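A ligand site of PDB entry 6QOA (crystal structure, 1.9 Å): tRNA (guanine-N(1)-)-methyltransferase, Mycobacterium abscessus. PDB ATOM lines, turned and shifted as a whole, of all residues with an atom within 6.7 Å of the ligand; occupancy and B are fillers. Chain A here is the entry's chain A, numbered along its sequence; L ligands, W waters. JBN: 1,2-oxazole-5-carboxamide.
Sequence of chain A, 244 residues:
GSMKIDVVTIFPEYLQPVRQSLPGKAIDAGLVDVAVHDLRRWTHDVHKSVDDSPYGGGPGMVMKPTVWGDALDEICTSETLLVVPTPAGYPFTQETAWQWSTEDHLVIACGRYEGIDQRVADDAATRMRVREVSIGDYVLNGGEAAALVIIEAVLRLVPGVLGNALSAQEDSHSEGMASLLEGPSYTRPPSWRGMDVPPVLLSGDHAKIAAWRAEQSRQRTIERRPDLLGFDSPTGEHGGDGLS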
ATOM      1  N   PRO A  85     -23.808 -14.512  -4.513  1.00  0.00           N
ATOM      2  CA  PRO A  85     -22.877 -14.646  -3.377  1.00  0.00           C
ATOM      3  C   PRO A  85     -23.632 -14.956  -2.091  1.00  0.00           C
ATOM      4  O   PRO A  85     -24.634 -14.319  -1.770  1.00  0.00           O
ATOM      5  CB  PRO A  85     -22.199 -13.285  -3.312  1.00  0.00           C
ATOM      6  CG  PRO A  85     -22.456 -12.644  -4.686  1.00  0.00           C
ATOM      7  CD  PRO A  85     -23.799 -13.153  -5.067  1.00  0.00           C
ATOM      8  N   THR A  86     -23.154 -15.959  -1.378  1.00  0.00           N
ATOM      9  CA  THR A  86     -23.802 -16.420  -0.173  1.00  0.00           C
ATOM     10  C   THR A  86     -22.824 -17.237   0.648  1.00  0.00           C
ATOM     11  O   THR A  86     -22.027 -17.999   0.109  1.00  0.00           O
ATOM     12  CB  THR A  86     -25.047 -17.276  -0.489  1.00  0.00           C
ATOM     13  OG1 THR A  86     -25.402 -17.990   0.699  1.00  0.00           O
ATOM     14  CG2 THR A  86     -24.744 -18.271  -1.591  1.00  0.00           C
ATOM     15  N   PRO A  87     -22.890 -17.097   1.965  1.00  0.00           N
ATOM     16  CA  PRO A  87     -22.009 -17.894   2.833  1.00  0.00           C
ATOM     17  C   PRO A  87     -22.301 -19.390   2.737  1.00  0.00           C
ATOM     18  O   PRO A  87     -21.497 -20.197   3.209  1.00  0.00           O
ATOM     19  CB  PRO A  87     -22.324 -17.367   4.241  1.00  0.00           C
ATOM     20  CG  PRO A  87     -23.654 -16.688   4.113  1.00  0.00           C
ATOM     21  CD  PRO A  87     -23.757 -16.172   2.722  1.00  0.00           C
ATOM     22  N   ALA A  88     -23.422 -19.756   2.118  1.00  0.00           N
ATOM     23  CA  ALA A  88     -23.733 -21.176   1.928  1.00  0.00           C
ATOM     24  C   ALA A  88     -23.296 -21.705   0.576  1.00  0.00           C
ATOM     25  O   ALA A  88     -23.652 -22.814   0.193  1.00  0.00           O
ATOM     26  CB  ALA A  88     -25.238 -21.422   2.100  1.00  0.00           C
ATOM     27  N   GLY A  89     -22.523 -20.913  -0.168  1.00  0.00           N
ATOM     28  CA  GLY A  89     -22.205 -21.270  -1.529  1.00  0.00           C
ATOM     29  C   GLY A  89     -21.009 -22.198  -1.671  1.00  0.00           C
ATOM     30  O   GLY A  89     -20.319 -22.488  -0.697  1.00  0.00           O
ATOM     31  N   GLY A 111     -27.935 -10.446  -2.324  1.00  0.00           N
ATOM     32  CA  GLY A 111     -29.014 -10.575  -1.363  1.00  0.00           C
ATOM     33  C   GLY A 111     -28.519 -10.600   0.071  1.00  0.00           C
ATOM     34  O   GLY A 111     -27.329 -10.817   0.317  1.00  0.00           O
ATOM     35  N   ARG A 112     -29.423 -10.401   1.017  1.00  0.00           N
ATOM     36  CA  ARG A 112     -29.093 -10.572   2.426  1.00  0.00           C
ATOM     37  C   ARG A 112     -28.707 -12.021   2.712  1.00  0.00           C
ATOM     38  O   ARG A 112     -29.154 -12.943   2.020  1.00  0.00           O
ATOM     39  CB  ARG A 112     -30.255 -10.137   3.317  1.00  0.00           C
ATOM     40  CG  ARG A 112     -31.533 -10.894   3.061  1.00  0.00           C
ATOM     41  CD  ARG A 112     -32.669 -10.289   3.901  1.00  0.00           C
ATOM     42  NE  ARG A 112     -32.356 -10.363   5.331  1.00  0.00           N
ATOM     43  CZ  ARG A 112     -32.738  -9.467   6.237  1.00  0.00           C
ATOM     44  NH1 ARG A 112     -32.415  -9.622   7.511  1.00  0.00           N
ATOM     45  NH2 ARG A 112     -33.450  -8.412   5.863  1.00  0.00           N
ATOM     46  N   TYR A 113     -27.881 -12.253   3.735  1.00  0.00           N
ATOM     47  CA  TYR A 113     -27.247 -13.552   3.894  1.00  0.00           C
ATOM     48  C   TYR A 113     -28.242 -14.650   4.296  1.00  0.00           C
ATOM     49  O   TYR A 113     -27.992 -15.832   4.039  1.00  0.00           O
ATOM     50  CB  TYR A 113     -26.103 -13.489   4.910  1.00  0.00           C
ATOM     51  CG  TYR A 113     -26.575 -13.625   6.336  1.00  0.00           C
ATOM     52  CD1 TYR A 113     -27.041 -12.524   7.040  1.00  0.00           C
ATOM     53  CD2 TYR A 113     -26.562 -14.859   6.969  1.00  0.00           C
ATOM     54  CE1 TYR A 113     -27.477 -12.647   8.345  1.00  0.00           C
ATOM     55  CE2 TYR A 113     -26.986 -14.989   8.271  1.00  0.00           C
ATOM     56  CZ  TYR A 113     -27.444 -13.883   8.953  1.00  0.00           C
ATOM     57  OH  TYR A 113     -27.869 -14.026  10.248  1.00  0.00           O
ATOM     58  N   VAL A 133     -21.998 -18.921  -4.645  1.00  0.00           N
ATOM     59  CA  VAL A 133     -20.600 -19.032  -4.233  1.00  0.00           C
ATOM     60  C   VAL A 133     -20.346 -18.232  -2.977  1.00  0.00           C
ATOM     61  O   VAL A 133     -20.969 -17.193  -2.764  1.00  0.00           O
ATOM     62  CB  VAL A 133     -19.639 -18.538  -5.328  1.00  0.00           C
ATOM     63  CG1 VAL A 133     -19.707 -19.457  -6.548  1.00  0.00           C
ATOM     64  CG2 VAL A 133     -19.953 -17.087  -5.735  1.00  0.00           C
ATOM     65  N   SER A 134     -19.444 -18.733  -2.134  1.00  0.00           N
ATOM     66  CA  SER A 134     -18.982 -18.028  -0.940  1.00  0.00           C
ATOM     67  C   SER A 134     -17.575 -17.518  -1.153  1.00  0.00           C
ATOM     68  O   SER A 134     -16.721 -18.255  -1.658  1.00  0.00           O
ATOM     69  CB  SER A 134     -19.024 -18.955   0.286  1.00  0.00           C
ATOM     70  OG  SER A 134     -18.294 -18.410   1.369  1.00  0.00           O
ATOM     71  N   ILE A 135     -17.290 -16.280  -0.782  1.00  0.00           N
ATOM     72  CA  ILE A 135     -15.918 -15.789  -0.932  1.00  0.00           C
ATOM     73  C   ILE A 135     -15.030 -16.091   0.294  1.00  0.00           C
ATOM     74  O   ILE A 135     -13.830 -15.749   0.301  1.00  0.00           O
ATOM     75  CB  ILE A 135     -15.889 -14.276  -1.212  1.00  0.00           C
ATOM     76  CG1 ILE A 135     -16.575 -13.518  -0.068  1.00  0.00           C
ATOM     77  CG2 ILE A 135     -16.526 -13.950  -2.604  1.00  0.00           C
ATOM     78  CD1 ILE A 135     -16.129 -12.063   0.035  1.00  0.00           C
ATOM     79  N   GLY A 136     -15.577 -16.743   1.310  1.00  0.00           N
ATOM     80  CA  GLY A 136     -14.815 -17.047   2.515  1.00  0.00           C
ATOM     81  C   GLY A 136     -15.661 -17.512   3.698  1.00  0.00           C
ATOM     82  O   GLY A 136     -16.886 -17.433   3.656  1.00  0.00           O
ATOM     83  N   ASP A 137     -15.026 -17.999   4.756  1.00  0.00           N
ATOM     84  CA  ASP A 137     -15.788 -18.573   5.863  1.00  0.00           C
ATOM     85  C   ASP A 137     -16.136 -17.530   6.918  1.00  0.00           C
ATOM     86  O   ASP A 137     -15.627 -17.556   8.040  1.00  0.00           O
ATOM     87  CB  ASP A 137     -15.017 -19.726   6.512  1.00  0.00           C
ATOM     88  CG  ASP A 137     -14.977 -20.947   5.637  1.00  0.00           C
ATOM     89  OD1 ASP A 137     -15.919 -21.135   4.840  1.00  0.00           O
ATOM     90  OD2 ASP A 137     -14.010 -21.714   5.750  1.00  0.00           O
ATOM     91  N   TYR A 138     -17.019 -16.614   6.550  1.00  0.00           N
ATOM     92  CA  TYR A 138     -17.486 -15.589   7.460  1.00  0.00           C
ATOM     93  C   TYR A 138     -18.799 -15.116   6.906  1.00  0.00           C
ATOM     94  O   TYR A 138     -19.100 -15.373   5.746  1.00  0.00           O
ATOM     95  CB  TYR A 138     -16.483 -14.438   7.568  1.00  0.00           C
ATOM     96  CG  TYR A 138     -15.839 -14.129   6.245  1.00  0.00           C
ATOM     97  CD1 TYR A 138     -16.521 -13.425   5.259  1.00  0.00           C
ATOM     98  CD2 TYR A 138     -14.556 -14.576   5.957  1.00  0.00           C
ATOM     99  CE1 TYR A 138     -15.936 -13.166   4.024  1.00  0.00           C
ATOM    100  CE2 TYR A 138     -13.956 -14.313   4.741  1.00  0.00           C
ATOM    101  CZ  TYR A 138     -14.647 -13.602   3.772  1.00  0.00           C
ATOM    102  OH  TYR A 138     -14.083 -13.363   2.547  1.00  0.00           O
ATOM    103  N   VAL A 139     -19.584 -14.431   7.721  1.00  0.00           N
ATOM    104  CA  VAL A 139     -20.882 -13.933   7.287  1.00  0.00           C
ATOM    105  C   VAL A 139     -20.844 -12.418   7.084  1.00  0.00           C
ATOM    106  O   VAL A 139     -20.320 -11.700   7.936  1.00  0.00           O
ATOM    107  CB  VAL A 139     -21.971 -14.289   8.309  1.00  0.00           C
ATOM    108  CG1 VAL A 139     -23.269 -13.538   8.018  1.00  0.00           C
ATOM    109  CG2 VAL A 139     -22.179 -15.791   8.349  1.00  0.00           C
ATOM    110  N   LEU A 140     -21.367 -11.950   5.962  1.00  0.00           N
ATOM    111  CA  LEU A 140     -21.616 -10.536   5.744  1.00  0.00           C
ATOM    112  C   LEU A 140     -23.125 -10.321   5.815  1.00  0.00           C
ATOM    113  O   LEU A 140     -23.883 -11.258   5.611  1.00  0.00           O
ATOM    114  CB  LEU A 140     -21.063 -10.062   4.406  1.00  0.00           C
ATOM    115  CG  LEU A 140     -19.684 -10.581   4.019  1.00  0.00           C
ATOM    116  CD1 LEU A 140     -19.337 -10.122   2.610  1.00  0.00           C
ATOM    117  CD2 LEU A 140     -18.630 -10.123   5.027  1.00  0.00           C
ATOM    118  N   ASN A 141     -23.579  -9.109   6.117  1.00  0.00           N
ATOM    119  CA  ASN A 141     -25.020  -8.861   6.112  1.00  0.00           C
ATOM    120  C   ASN A 141     -25.670  -9.146   4.770  1.00  0.00           C
ATOM    121  O   ASN A 141     -26.805  -9.595   4.712  1.00  0.00           O
ATOM    122  CB  ASN A 141     -25.328  -7.424   6.516  1.00  0.00           C
ATOM    123  CG  ASN A 141     -25.832  -7.323   7.940  1.00  0.00           C
ATOM    124  OD1 ASN A 141     -25.561  -8.205   8.766  1.00  0.00           O
ATOM    125  ND2 ASN A 141     -26.595  -6.270   8.229  1.00  0.00           N
ATOM    126  N   GLY A 142     -24.946  -8.868   3.690  1.00  0.00           N
ATOM    127  CA  GLY A 142     -25.450  -9.116   2.351  1.00  0.00           C
ATOM    128  C   GLY A 142     -24.310  -9.410   1.396  1.00  0.00           C
ATOM    129  O   GLY A 142     -23.141  -9.302   1.777  1.00  0.00           O
ATOM    130  N   GLY A 143     -24.662  -9.760   0.164  1.00  0.00           N
ATOM    131  CA  GLY A 143     -23.696 -10.115  -0.862  1.00  0.00           C
ATOM    132  C   GLY A 143     -22.954  -8.958  -1.519  1.00  0.00           C
ATOM    133  O   GLY A 143     -22.112  -9.182  -2.389  1.00  0.00           O
ATOM    134  N   GLU A 144     -23.248  -7.721  -1.101  1.00  0.00           N
ATOM    135  CA  GLU A 144     -22.646  -6.556  -1.754  1.00  0.00           C
ATOM    136  C   GLU A 144     -21.115  -6.537  -1.722  1.00  0.00           C
ATOM    137  O   GLU A 144     -20.471  -6.393  -2.748  1.00  0.00           O
ATOM    138  CB  GLU A 144     -23.179  -5.263  -1.126  1.00  0.00           C
ATOM    139  CG  GLU A 144     -24.547  -4.812  -1.664  1.00  0.00           C
ATOM    140  CD  GLU A 144     -25.697  -5.668  -1.162  1.00  0.00           C
ATOM    141  OE1 GLU A 144     -25.541  -6.294  -0.086  1.00  0.00           O
ATOM    142  OE2 GLU A 144     -26.761  -5.679  -1.825  1.00  0.00           O
ATOM    143  N   ALA A 146     -19.118  -8.945  -1.172  1.00  0.00           N
ATOM    144  CA  ALA A 146     -18.631 -10.122  -1.903  1.00  0.00           C
ATOM    145  C   ALA A 146     -18.664  -9.903  -3.415  1.00  0.00           C
ATOM    146  O   ALA A 146     -17.799 -10.404  -4.146  1.00  0.00           O
ATOM    147  CB  ALA A 146     -19.441 -11.344  -1.538  1.00  0.00           C
HETATM  148  O01 JBN L   1     -19.428 -15.071   0.530  1.00  0.00           O
HETATM  149  C02 JBN L   1     -19.768 -14.958   1.694  1.00  0.00           C
HETATM  150  N03 JBN L   1     -19.038 -15.605   2.730  1.00  0.00           N
HETATM  151  C04 JBN L   1     -20.977 -14.135   2.036  1.00  0.00           C
HETATM  152  O05 JBN L   1     -21.365 -13.826   3.294  1.00  0.00           O
HETATM  153  N06 JBN L   1     -22.531 -13.061   3.181  1.00  0.00           N
HETATM  154  C07 JBN L   1     -22.848 -12.913   1.877  1.00  0.00           C
HETATM  155  C08 JBN L   1     -21.881 -13.579   1.130  1.00  0.00           C
HETATM  156  O   HOH W   1     -25.875 -13.237   0.656  1.00  0.00           O
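The backbone NH (N) of Ile 135 sits at hydrogen-bond distance from an oxygen (O01) of the ligand.
A nitrogen (N03) of the ligand is in hydrogen-bond range of the backbone carbonyl oxygen (O) of Gly 136 (3.0 Å).
The backbone carbonyl oxygen of Tyr 138 sits at hydrogen-bond distance from a nitrogen (N03) of the ligand (3.0 Å).
A nitrogen (N03) of the ligand lies within hydrogen-bond range of the side-chain hydroxyl (OG) of Ser 134, 3.2 Å away.
The backbone NH of Leu 140 lies within hydrogen-bond range of a nitrogen (N06) of the ligand (3.2 Å).
Residues that only touch the ligand: Pro 85, Thr 86, Pro 87, Tyr 113 and Gly 142.
Hydrophobic or aromatic side chains within 4 Å of the ligand: Pro 87, Tyr 113, Ile 135 and Leu 140.
The backbone carbonyl oxygen (O) of Ile 135 sits at hydrogen-bond distance from the side-chain hydroxyl (OH) of Tyr 138, 3.3 Å away.
O of Gly 136 is in hydrogen-bond range of OG of Ser 134 (2.9 Å).
The backbone NH (N) of Ser 134 lies close to the backbone carbonyl oxygen (O) of Thr 86 (3.5 Å).
N of Thr 86 sits at hydrogen-bond distance from O of Val 133 (2.9 Å).
The side-chain hydroxyl of Thr 86 lies close to the backbone NH of Ala 88.
The backbone NH (N) of Tyr 113 lies within hydrogen-bond range of the backbone carbonyl oxygen (O) of Asn 141 (3.0 Å).
Water W1 bridges O of Gly 111 (2.8 Å) and O of Pro 85 (2.9 Å).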
